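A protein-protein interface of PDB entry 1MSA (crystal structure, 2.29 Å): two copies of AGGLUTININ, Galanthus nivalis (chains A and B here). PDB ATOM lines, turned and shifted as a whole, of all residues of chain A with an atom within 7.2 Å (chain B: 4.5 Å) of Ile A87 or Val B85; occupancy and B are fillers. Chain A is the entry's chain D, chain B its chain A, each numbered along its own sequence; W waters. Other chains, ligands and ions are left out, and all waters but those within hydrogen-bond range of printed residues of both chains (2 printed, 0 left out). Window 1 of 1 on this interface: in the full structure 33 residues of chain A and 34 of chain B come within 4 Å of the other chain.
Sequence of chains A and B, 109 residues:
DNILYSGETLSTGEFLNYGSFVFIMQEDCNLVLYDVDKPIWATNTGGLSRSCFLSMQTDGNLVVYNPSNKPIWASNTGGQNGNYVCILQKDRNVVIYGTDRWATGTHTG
O of Val A85 is in hydrogen-bond range of N of Tyr A97 (2.9 Å).
The side-chain hydroxyl of Tyr A97 sits at hydrogen-bond distance from the side-chain amide oxygen of Gln A89 (2.6 Å).
N of Ile B87 is in hydrogen-bond range of O of Val B95 (2.9 Å).
The backbone NH (N) of Ile A87 is in hydrogen-bond range of the backbone carbonyl oxygen (O) of Val A95.
O of Asn A2 sits at hydrogen-bond distance from N of Leu A88, 2.7 Å away.
NE2 of Gln A89 is in hydrogen-bond range of OD1 of Asp A91.
Ile A3 touches Ile B87, and with the chains exchanged Ile A87 touches Ile B3.
Val A85 touches Tyr B97, and with the chains exchanged Tyr A97 touches Val B85.
Ile A87 touches Val B85, but with the chains exchanged Val A85 does not touch Ile B87 (4.04 Å).
Ile B87 touches its own counterpart, Ile A87.
Positions printed for both chains: 3, 4, 56, 85, 86, 87, 95, 96 and 97.
Water W2 bridges the side-chain amino group of Lys A90 (2.7 Å) and the backbone carbonyl oxygen of Ile B3 (3.4 Å).
Water W1 bridges O of Tyr B84 (2.9 Å) and OH of Tyr A97 (3.0 Å).
Hydrophobic or aromatic side chains of chain A within 4 Å of the printed part of chain B: Ile A3, Val A85, Ile A87, Tyr A97 and Trp A102.
Of the 11 printed residues of chain B, 7 touch a printed residue of chain A.
Hydrophobic or aromatic side chains of chain B that line the printed part of chain A: Ile B3, Tyr B5, Val B85, Ile B87, Val B95, Ile B96 and Tyr B97.
Among the printed residues, 12 pairs touch across the chains.
Among the printed residues, no Asp or Glu carboxylate lies within 4 Å of a Lys or Arg side-chain nitrogen of the other chain.
Met A56 touches none of the printed residues of chain B.
Printed residues of chain B within 4 Å of Val A85: Tyr B97.
Printed residues of chain B within 4 Å of Gln A89: Tyr B5.
Leu B4 touches none of the printed residues of chain A.
Of chain A, only Ile A87 (3.95 Å) and Tyr A97 (3.9 Å) come within 4 Å of Val B85.
The nearest residue of chain A that does not touch Val B85 is Gln A89 (4.6 Å).
The nearest printed residue of chain B that does not touch Ile A3 is Ile B3 (4.1 Å).
The backbone NH (N) of Ile B96 lies within hydrogen-bond range of the backbone carbonyl oxygen (O) of Trp A102, 2.8 Å away.
Among the printed residues, pairs that only touch across the chains: Trp A102 with Val B95 (3.2 Å), Asn A2 with Ile B3 (3.4 Å), Gln A89 with Tyr B5 (3.5 Å), Lys A90 with Tyr B5 (3.7 Å), Val A85 with Tyr B97 (3.8 Å), Ile A87 with Ile B3 (3.8 Å), Ile A3 with Ile B87 (3.8 Å), Tyr A97 with Tyr B97 (3.8 Å), Ile A87 with Ile B87 (3.8 Å), Tyr A97 with Val B85 (3.9 Å) and Ile A87 with Val B85 (3.95 Å).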
ATOM      1  N   ASN A   2      18.393  12.035  24.671  1.00  0.00           N
ATOM      2  CA  ASN A   2      18.010  13.421  24.465  1.00  0.00           C
ATOM      3  C   ASN A   2      16.513  13.591  24.251  1.00  0.00           C
ATOM      4  O   ASN A   2      16.042  14.707  24.001  1.00  0.00           O
ATOM      5  CB  ASN A   2      18.779  14.016  23.284  1.00  0.00           C
ATOM      6  CG  ASN A   2      18.487  13.346  21.963  1.00  0.00           C
ATOM      7  OD1 ASN A   2      18.226  12.142  21.880  1.00  0.00           O
ATOM      8  ND2 ASN A   2      18.537  14.126  20.884  1.00  0.00           N
ATOM      9  N   ILE A   3      15.750  12.508  24.333  1.00  0.00           N
ATOM     10  CA  ILE A   3      14.320  12.543  24.114  1.00  0.00           C
ATOM     11  C   ILE A   3      13.519  11.979  25.288  1.00  0.00           C
ATOM     12  O   ILE A   3      13.829  10.917  25.813  1.00  0.00           O
ATOM     13  CB  ILE A   3      13.897  11.727  22.867  1.00  0.00           C
ATOM     14  CG1 ILE A   3      14.636  12.179  21.614  1.00  0.00           C
ATOM     15  CG2 ILE A   3      12.391  11.848  22.658  1.00  0.00           C
ATOM     16  CD1 ILE A   3      14.471  11.263  20.424  1.00  0.00           C
ATOM     17  N   LEU A   4      12.469  12.699  25.663  1.00  0.00           N
ATOM     18  CA  LEU A   4      11.545  12.239  26.702  1.00  0.00           C
ATOM     19  C   LEU A   4      10.194  12.018  26.001  1.00  0.00           C
ATOM     20  O   LEU A   4       9.670  12.971  25.415  1.00  0.00           O
ATOM     21  CB  LEU A   4      11.410  13.240  27.833  1.00  0.00           C
ATOM     22  CG  LEU A   4      10.500  12.848  29.004  1.00  0.00           C
ATOM     23  CD1 LEU A   4      11.093  11.677  29.779  1.00  0.00           C
ATOM     24  CD2 LEU A   4      10.254  14.024  29.932  1.00  0.00           C
ATOM     25  N   LEU A  16      18.114  14.554  30.647  1.00  0.00           N
ATOM     26  CA  LEU A  16      18.231  14.349  29.206  1.00  0.00           C
ATOM     27  C   LEU A  16      19.629  14.917  28.875  1.00  0.00           C
ATOM     28  O   LEU A  16      19.983  15.916  29.522  1.00  0.00           O
ATOM     29  CB  LEU A  16      17.186  15.110  28.420  1.00  0.00           C
ATOM     30  CG  LEU A  16      15.728  14.672  28.520  1.00  0.00           C
ATOM     31  CD1 LEU A  16      14.858  15.520  27.602  1.00  0.00           C
ATOM     32  CD2 LEU A  16      15.573  13.190  28.205  1.00  0.00           C
ATOM     33  N   PHE A  23      19.901  18.463  30.800  1.00  0.00           N
ATOM     34  CA  PHE A  23      18.583  18.954  31.282  1.00  0.00           C
ATOM     35  C   PHE A  23      18.197  18.037  32.443  1.00  0.00           C
ATOM     36  O   PHE A  23      17.776  16.898  32.213  1.00  0.00           O
ATOM     37  CB  PHE A  23      17.603  18.863  30.136  1.00  0.00           C
ATOM     38  CG  PHE A  23      16.267  19.505  30.300  1.00  0.00           C
ATOM     39  CD1 PHE A  23      16.151  20.862  30.553  1.00  0.00           C
ATOM     40  CD2 PHE A  23      15.107  18.757  30.164  1.00  0.00           C
ATOM     41  CE1 PHE A  23      14.912  21.459  30.680  1.00  0.00           C
ATOM     42  CE2 PHE A  23      13.862  19.347  30.275  1.00  0.00           C
ATOM     43  CZ  PHE A  23      13.767  20.701  30.528  1.00  0.00           C
ATOM     44  N   MET A  56       6.270  13.963  31.248  1.00  0.00           N
ATOM     45  CA  MET A  56       5.854  14.413  29.909  1.00  0.00           C
ATOM     46  C   MET A  56       4.531  13.690  29.613  1.00  0.00           C
ATOM     47  O   MET A  56       4.536  12.497  29.303  1.00  0.00           O
ATOM     48  CB  MET A  56       6.894  14.078  28.867  1.00  0.00           C
ATOM     49  CG  MET A  56       6.461  14.275  27.420  1.00  0.00           C
ATOM     50  SD  MET A  56       6.427  16.012  26.945  1.00  0.00           S
ATOM     51  CE  MET A  56       4.711  16.418  27.183  1.00  0.00           C
ATOM     52  N   VAL A  85       6.706  14.412  22.155  1.00  0.00           N
ATOM     53  CA  VAL A  85       8.091  14.209  22.523  1.00  0.00           C
ATOM     54  C   VAL A  85       8.702  15.516  23.057  1.00  0.00           C
ATOM     55  O   VAL A  85       8.396  16.591  22.545  1.00  0.00           O
ATOM     56  CB  VAL A  85       9.007  13.760  21.369  1.00  0.00           C
ATOM     57  CG1 VAL A  85       8.808  12.310  21.003  1.00  0.00           C
ATOM     58  CG2 VAL A  85       8.842  14.680  20.170  1.00  0.00           C
ATOM     59  N   CYS A  86       9.563  15.379  24.047  1.00  0.00           N
ATOM     60  CA  CYS A  86      10.301  16.531  24.582  1.00  0.00           C
ATOM     61  C   CYS A  86      11.773  16.247  24.241  1.00  0.00           C
ATOM     62  O   CYS A  86      12.298  15.200  24.624  1.00  0.00           O
ATOM     63  CB  CYS A  86      10.104  16.722  26.067  1.00  0.00           C
ATOM     64  SG  CYS A  86      11.072  18.077  26.785  1.00  0.00           S
ATOM     65  N   ILE A  87      12.365  17.097  23.419  1.00  0.00           N
ATOM     66  CA  ILE A  87      13.706  16.875  22.928  1.00  0.00           C
ATOM     67  C   ILE A  87      14.730  17.908  23.355  1.00  0.00           C
ATOM     68  O   ILE A  87      14.500  19.105  23.240  1.00  0.00           O
ATOM     69  CB  ILE A  87      13.693  16.875  21.366  1.00  0.00           C
ATOM     70  CG1 ILE A  87      12.716  15.830  20.839  1.00  0.00           C
ATOM     71  CG2 ILE A  87      15.088  16.632  20.818  1.00  0.00           C
ATOM     72  CD1 ILE A  87      12.505  15.878  19.337  1.00  0.00           C
ATOM     73  N   LEU A  88      15.885  17.414  23.817  1.00  0.00           N
ATOM     74  CA  LEU A  88      17.017  18.314  24.095  1.00  0.00           C
ATOM     75  C   LEU A  88      17.819  18.275  22.766  1.00  0.00           C
ATOM     76  O   LEU A  88      18.445  17.275  22.448  1.00  0.00           O
ATOM     77  CB  LEU A  88      17.858  17.906  25.268  1.00  0.00           C
ATOM     78  CG  LEU A  88      19.253  18.535  25.391  1.00  0.00           C
ATOM     79  CD1 LEU A  88      19.179  20.053  25.437  1.00  0.00           C
ATOM     80  CD2 LEU A  88      19.978  18.003  26.617  1.00  0.00           C
ATOM     81  N   GLN A  89      17.596  19.290  21.946  1.00  0.00           N
ATOM     82  CA  GLN A  89      18.163  19.368  20.622  1.00  0.00           C
ATOM     83  C   GLN A  89      19.625  19.733  20.576  1.00  0.00           C
ATOM     84  O   GLN A  89      20.192  20.301  21.507  1.00  0.00           O
ATOM     85  CB  GLN A  89      17.352  20.386  19.772  1.00  0.00           C
ATOM     86  CG  GLN A  89      15.873  20.037  19.729  1.00  0.00           C
ATOM     87  CD  GLN A  89      15.049  20.863  18.779  1.00  0.00           C
ATOM     88  OE1 GLN A  89      13.901  20.517  18.467  1.00  0.00           O
ATOM     89  NE2 GLN A  89      15.587  21.972  18.290  1.00  0.00           N
ATOM     90  N   LYS A  90      20.241  19.480  19.412  1.00  0.00           N
ATOM     91  CA  LYS A  90      21.643  19.788  19.188  1.00  0.00           C
ATOM     92  C   LYS A  90      21.911  21.281  19.149  1.00  0.00           C
ATOM     93  O   LYS A  90      23.041  21.713  19.394  1.00  0.00           O
ATOM     94  CB  LYS A  90      22.136  19.123  17.902  1.00  0.00           C
ATOM     95  CG  LYS A  90      21.395  19.584  16.657  1.00  0.00           C
ATOM     96  CD  LYS A  90      21.753  18.708  15.469  1.00  0.00           C
ATOM     97  CE  LYS A  90      21.248  19.317  14.172  1.00  0.00           C
ATOM     98  NZ  LYS A  90      21.354  18.351  13.042  1.00  0.00           N
ATOM     99  N   ASP A  91      20.885  22.097  18.905  1.00  0.00           N
ATOM    100  CA  ASP A  91      21.039  23.543  18.885  1.00  0.00           C
ATOM    101  C   ASP A  91      20.866  24.147  20.273  1.00  0.00           C
ATOM    102  O   ASP A  91      20.814  25.368  20.431  1.00  0.00           O
ATOM    103  CB  ASP A  91      20.098  24.194  17.890  1.00  0.00           C
ATOM    104  CG  ASP A  91      18.632  24.065  18.207  1.00  0.00           C
ATOM    105  OD1 ASP A  91      18.249  23.379  19.178  1.00  0.00           O
ATOM    106  OD2 ASP A  91      17.822  24.667  17.459  1.00  0.00           O
ATOM    107  N   ARG A  92      20.727  23.312  21.286  1.00  0.00           N
ATOM    108  CA  ARG A  92      20.605  23.676  22.664  1.00  0.00           C
ATOM    109  C   ARG A  92      19.211  24.075  23.103  1.00  0.00           C
ATOM    110  O   ARG A  92      19.008  24.432  24.269  1.00  0.00           O
ATOM    111  CB  ARG A  92      21.613  24.751  23.088  1.00  0.00           C
ATOM    112  CG  ARG A  92      21.905  24.707  24.592  1.00  0.00           C
ATOM    113  CD  ARG A  92      22.970  25.730  24.960  1.00  0.00           C
ATOM    114  NE  ARG A  92      22.480  27.089  24.777  1.00  0.00           N
ATOM    115  CZ  ARG A  92      23.197  28.184  25.000  1.00  0.00           C
ATOM    116  NH1 ARG A  92      24.455  28.082  25.414  1.00  0.00           N
ATOM    117  NH2 ARG A  92      22.654  29.379  24.802  1.00  0.00           N
ATOM    118  N   ASN A  93      18.240  23.982  22.211  1.00  0.00           N
ATOM    119  CA  ASN A  93      16.859  24.311  22.529  1.00  0.00           C
ATOM    120  C   ASN A  93      16.110  23.073  23.012  1.00  0.00           C
ATOM    121  O   ASN A  93      16.314  21.981  22.482  1.00  0.00           O
ATOM    122  CB  ASN A  93      16.155  24.864  21.280  1.00  0.00           C
ATOM    123  CG  ASN A  93      15.032  25.811  21.646  1.00  0.00           C
ATOM    124  OD1 ASN A  93      14.886  26.192  22.808  1.00  0.00           O
ATOM    125  ND2 ASN A  93      14.234  26.198  20.659  1.00  0.00           N
ATOM    126  N   VAL A  94      15.281  23.244  24.031  1.00  0.00           N
ATOM    127  CA  VAL A  94      14.463  22.126  24.529  1.00  0.00           C
ATOM    128  C   VAL A  94      13.047  22.379  24.001  1.00  0.00           C
ATOM    129  O   VAL A  94      12.452  23.402  24.339  1.00  0.00           O
ATOM    130  CB  VAL A  94      14.459  22.020  26.050  1.00  0.00           C
ATOM    131  CG1 VAL A  94      13.596  20.853  26.516  1.00  0.00           C
ATOM    132  CG2 VAL A  94      15.878  21.867  26.594  1.00  0.00           C
ATOM    133  N   VAL A  95      12.583  21.543  23.081  1.00  0.00           N
ATOM    134  CA  VAL A  95      11.288  21.744  22.453  1.00  0.00           C
ATOM    135  C   VAL A  95      10.348  20.559  22.620  1.00  0.00           C
ATOM    136  O   VAL A  95      10.772  19.403  22.616  1.00  0.00           O
ATOM    137  CB  VAL A  95      11.452  21.972  20.923  1.00  0.00           C
ATOM    138  CG1 VAL A  95      10.155  22.469  20.304  1.00  0.00           C
ATOM    139  CG2 VAL A  95      12.591  22.920  20.607  1.00  0.00           C
ATOM    140  N   ILE A  96       9.048  20.858  22.699  1.00  0.00           N
ATOM    141  CA  ILE A  96       8.023  19.820  22.762  1.00  0.00           C
ATOM    142  C   ILE A  96       7.341  19.769  21.382  1.00  0.00           C
ATOM    143  O   ILE A  96       6.939  20.814  20.864  1.00  0.00           O
ATOM    144  CB  ILE A  96       6.962  20.073  23.831  1.00  0.00           C
ATOM    145  CG1 ILE A  96       7.556  20.044  25.240  1.00  0.00           C
ATOM    146  CG2 ILE A  96       5.818  19.058  23.718  1.00  0.00           C
ATOM    147  CD1 ILE A  96       6.597  20.506  26.325  1.00  0.00           C
ATOM    148  N   TYR A  97       7.293  18.588  20.789  1.00  0.00           N
ATOM    149  CA  TYR A  97       6.676  18.404  19.484  1.00  0.00           C
ATOM    150  C   TYR A  97       5.513  17.404  19.594  1.00  0.00           C
ATOM    151  O   TYR A  97       5.571  16.481  20.403  1.00  0.00           O
ATOM    152  CB  TYR A  97       7.650  17.846  18.451  1.00  0.00           C
ATOM    153  CG  TYR A  97       8.779  18.751  18.046  1.00  0.00           C
ATOM    154  CD1 TYR A  97       9.990  18.734  18.729  1.00  0.00           C
ATOM    155  CD2 TYR A  97       8.658  19.601  16.948  1.00  0.00           C
ATOM    156  CE1 TYR A  97      11.034  19.562  18.354  1.00  0.00           C
ATOM    157  CE2 TYR A  97       9.698  20.427  16.566  1.00  0.00           C
ATOM    158  CZ  TYR A  97      10.881  20.405  17.271  1.00  0.00           C
ATOM    159  OH  TYR A  97      11.922  21.227  16.897  1.00  0.00           O
ATOM    160  N   GLY A  98       4.519  17.576  18.731  1.00  0.00           N
ATOM    161  CA  GLY A  98       3.375  16.668  18.731  1.00  0.00           C
ATOM    162  C   GLY A  98       2.162  17.334  18.092  1.00  0.00           C
ATOM    163  O   GLY A  98       2.142  18.554  17.915  1.00  0.00           O
ATOM    164  N   TRP A 102       2.842  11.016  11.238  1.00  0.00           N
ATOM    165  CA  TRP A 102       3.059   9.856  10.363  1.00  0.00           C
ATOM    166  C   TRP A 102       4.038   8.902  11.034  1.00  0.00           C
ATOM    167  O   TRP A 102       4.811   9.324  11.906  1.00  0.00           O
ATOM    168  CB  TRP A 102       3.600  10.360   9.028  1.00  0.00           C
ATOM    169  CG  TRP A 102       4.025   9.317   8.051  1.00  0.00           C
ATOM    170  CD1 TRP A 102       3.259   8.752   7.068  1.00  0.00           C
ATOM    171  CD2 TRP A 102       5.325   8.722   7.933  1.00  0.00           C
ATOM    172  NE1 TRP A 102       3.999   7.837   6.358  1.00  0.00           N
ATOM    173  CE2 TRP A 102       5.274   7.804   6.869  1.00  0.00           C
ATOM    174  CE3 TRP A 102       6.531   8.887   8.623  1.00  0.00           C
ATOM    175  CZ2 TRP A 102       6.377   7.045   6.482  1.00  0.00           C
ATOM    176  CZ3 TRP A 102       7.629   8.142   8.230  1.00  0.00           C
ATOM    177  CH2 TRP A 102       7.541   7.226   7.174  1.00  0.00           C
ATOM    178  N   ILE B   3      17.594  11.810  14.923  1.00  0.00           N
ATOM    179  CA  ILE B   3      16.616  12.827  14.599  1.00  0.00           C
ATOM    180  C   ILE B   3      16.959  13.568  13.303  1.00  0.00           C
ATOM    181  O   ILE B   3      18.095  13.950  13.054  1.00  0.00           O
ATOM    182  CB  ILE B   3      16.485  13.888  15.711  1.00  0.00           C
ATOM    183  CG1 ILE B   3      16.113  13.263  17.054  1.00  0.00           C
ATOM    184  CG2 ILE B   3      15.453  14.942  15.324  1.00  0.00           C
ATOM    185  CD1 ILE B   3      16.337  14.188  18.233  1.00  0.00           C
ATOM    186  N   LEU B   4      15.937  13.779  12.490  1.00  0.00           N
ATOM    187  CA  LEU B   4      16.062  14.548  11.251  1.00  0.00           C
ATOM    188  C   LEU B   4      15.117  15.753  11.389  1.00  0.00           C
ATOM    189  O   LEU B   4      13.898  15.572  11.434  1.00  0.00           O
ATOM    190  CB  LEU B   4      15.728  13.710  10.041  1.00  0.00           C
ATOM    191  CG  LEU B   4      15.932  14.287   8.646  1.00  0.00           C
ATOM    192  CD1 LEU B   4      17.360  14.757   8.430  1.00  0.00           C
ATOM    193  CD2 LEU B   4      15.545  13.256   7.589  1.00  0.00           C
ATOM    194  N   TYR B   5      15.687  16.940  11.549  1.00  0.00           N
ATOM    195  CA  TYR B   5      14.904  18.146  11.742  1.00  0.00           C
ATOM    196  C   TYR B   5      14.342  18.715  10.449  1.00  0.00           C
ATOM    197  O   TYR B   5      14.977  18.643   9.397  1.00  0.00           O
ATOM    198  CB  TYR B   5      15.769  19.231  12.418  1.00  0.00           C
ATOM    199  CG  TYR B   5      16.277  18.815  13.780  1.00  0.00           C
ATOM    200  CD1 TYR B   5      17.459  18.095  13.903  1.00  0.00           C
ATOM    201  CD2 TYR B   5      15.564  19.111  14.934  1.00  0.00           C
ATOM    202  CE1 TYR B   5      17.922  17.689  15.145  1.00  0.00           C
ATOM    203  CE2 TYR B   5      16.021  18.713  16.179  1.00  0.00           C
ATOM    204  CZ  TYR B   5      17.198  18.000  16.274  1.00  0.00           C
ATOM    205  OH  TYR B   5      17.660  17.593  17.506  1.00  0.00           O
ATOM    206  N   MET B  56      13.241  16.303   5.038  1.00  0.00           N
ATOM    207  CA  MET B  56      12.196  16.541   6.054  1.00  0.00           C
ATOM    208  C   MET B  56      11.836  18.031   5.909  1.00  0.00           C
ATOM    209  O   MET B  56      12.637  18.883   6.295  1.00  0.00           O
ATOM    210  CB  MET B  56      12.687  16.239   7.447  1.00  0.00           C
ATOM    211  CG  MET B  56      11.750  16.577   8.585  1.00  0.00           C
ATOM    212  SD  MET B  56      10.278  15.555   8.660  1.00  0.00           S
ATOM    213  CE  MET B  56       8.997  16.710   8.236  1.00  0.00           C
ATOM    214  N   TYR B  84       9.175  20.602  12.449  1.00  0.00           N
ATOM    215  CA  TYR B  84       8.869  19.186  12.578  1.00  0.00           C
ATOM    216  C   TYR B  84      10.156  18.392  12.801  1.00  0.00           C
ATOM    217  O   TYR B  84      11.250  18.904  12.576  1.00  0.00           O
ATOM    218  CB  TYR B  84       8.205  18.653  11.302  1.00  0.00           C
ATOM    219  CG  TYR B  84       6.858  19.250  10.983  1.00  0.00           C
ATOM    220  CD1 TYR B  84       6.759  20.439  10.264  1.00  0.00           C
ATOM    221  CD2 TYR B  84       5.681  18.628  11.377  1.00  0.00           C
ATOM    222  CE1 TYR B  84       5.532  21.003   9.974  1.00  0.00           C
ATOM    223  CE2 TYR B  84       4.449  19.178  11.078  1.00  0.00           C
ATOM    224  CZ  TYR B  84       4.382  20.366  10.381  1.00  0.00           C
ATOM    225  OH  TYR B  84       3.152  20.911  10.078  1.00  0.00           O
ATOM    226  N   VAL B  85      10.018  17.157  13.258  1.00  0.00           N
ATOM    227  CA  VAL B  85      11.150  16.279  13.464  1.00  0.00           C
ATOM    228  C   VAL B  85      10.761  14.845  13.050  1.00  0.00           C
ATOM    229  O   VAL B  85       9.655  14.384  13.331  1.00  0.00           O
ATOM    230  CB  VAL B  85      11.683  16.209  14.898  1.00  0.00           C
ATOM    231  CG1 VAL B  85      12.452  17.448  15.303  1.00  0.00           C
ATOM    232  CG2 VAL B  85      10.571  15.898  15.889  1.00  0.00           C
ATOM    233  N   CYS B  86      11.680  14.202  12.357  1.00  0.00           N
ATOM    234  CA  CYS B  86      11.479  12.793  11.978  1.00  0.00           C
ATOM    235  C   CYS B  86      12.403  12.004  12.915  1.00  0.00           C
ATOM    236  O   CYS B  86      13.611  12.284  12.926  1.00  0.00           O
ATOM    237  CB  CYS B  86      11.826  12.553  10.523  1.00  0.00           C
ATOM    238  SG  CYS B  86      11.643  10.827  10.020  1.00  0.00           S
ATOM    239  N   ILE B  87      11.842  11.165  13.767  1.00  0.00           N
ATOM    240  CA  ILE B  87      12.639  10.464  14.755  1.00  0.00           C
ATOM    241  C   ILE B  87      12.713   8.958  14.606  1.00  0.00           C
ATOM    242  O   ILE B  87      11.682   8.284  14.582  1.00  0.00           O
ATOM    243  CB  ILE B  87      12.059  10.749  16.175  1.00  0.00           C
ATOM    244  CG1 ILE B  87      12.036  12.247  16.453  1.00  0.00           C
ATOM    245  CG2 ILE B  87      12.872  10.011  17.226  1.00  0.00           C
ATOM    246  CD1 ILE B  87      11.313  12.623  17.729  1.00  0.00           C
ATOM    247  N   VAL B  95       8.810   8.031  13.330  1.00  0.00           N
ATOM    248  CA  VAL B  95       7.653   8.894  13.458  1.00  0.00           C
ATOM    249  C   VAL B  95       7.954  10.366  13.191  1.00  0.00           C
ATOM    250  O   VAL B  95       9.015  10.878  13.537  1.00  0.00           O
ATOM    251  CB  VAL B  95       7.065   8.831  14.896  1.00  0.00           C
ATOM    252  CG1 VAL B  95       5.693   9.496  14.946  1.00  0.00           C
ATOM    253  CG2 VAL B  95       6.990   7.416  15.428  1.00  0.00           C
ATOM    254  N   ILE B  96       6.962  11.048  12.613  1.00  0.00           N
ATOM    255  CA  ILE B  96       7.070  12.484  12.372  1.00  0.00           C
ATOM    256  C   ILE B  96       6.181  13.197  13.405  1.00  0.00           C
ATOM    257  O   ILE B  96       5.015  12.824  13.554  1.00  0.00           O
ATOM    258  CB  ILE B  96       6.628  12.883  10.961  1.00  0.00           C
ATOM    259  CG1 ILE B  96       7.586  12.324   9.906  1.00  0.00           C
ATOM    260  CG2 ILE B  96       6.527  14.404  10.834  1.00  0.00           C
ATOM    261  CD1 ILE B  96       7.056  12.383   8.491  1.00  0.00           C
ATOM    262  N   TYR B  97       6.749  14.139  14.135  1.00  0.00           N
ATOM    263  CA  TYR B  97       6.004  14.887  15.140  1.00  0.00           C
ATOM    264  C   TYR B  97       6.035  16.382  14.777  1.00  0.00           C
ATOM    265  O   TYR B  97       7.040  16.853  14.245  1.00  0.00           O
ATOM    266  CB  TYR B  97       6.590  14.740  16.538  1.00  0.00           C
ATOM    267  CG  TYR B  97       6.541  13.384  17.178  1.00  0.00           C
ATOM    268  CD1 TYR B  97       7.579  12.474  17.016  1.00  0.00           C
ATOM    269  CD2 TYR B  97       5.472  13.008  17.987  1.00  0.00           C
ATOM    270  CE1 TYR B  97       7.547  11.227  17.619  1.00  0.00           C
ATOM    271  CE2 TYR B  97       5.429  11.765  18.593  1.00  0.00           C
ATOM    272  CZ  TYR B  97       6.476  10.884  18.411  1.00  0.00           C
ATOM    273  OH  TYR B  97       6.435   9.646  19.012  1.00  0.00           O
HETATM  274  O   HOH W   1      12.557  21.080  14.018  1.00  0.00           O
HETATM  275  O   HOH W   2      20.994  15.740  13.344  1.00  0.00           O
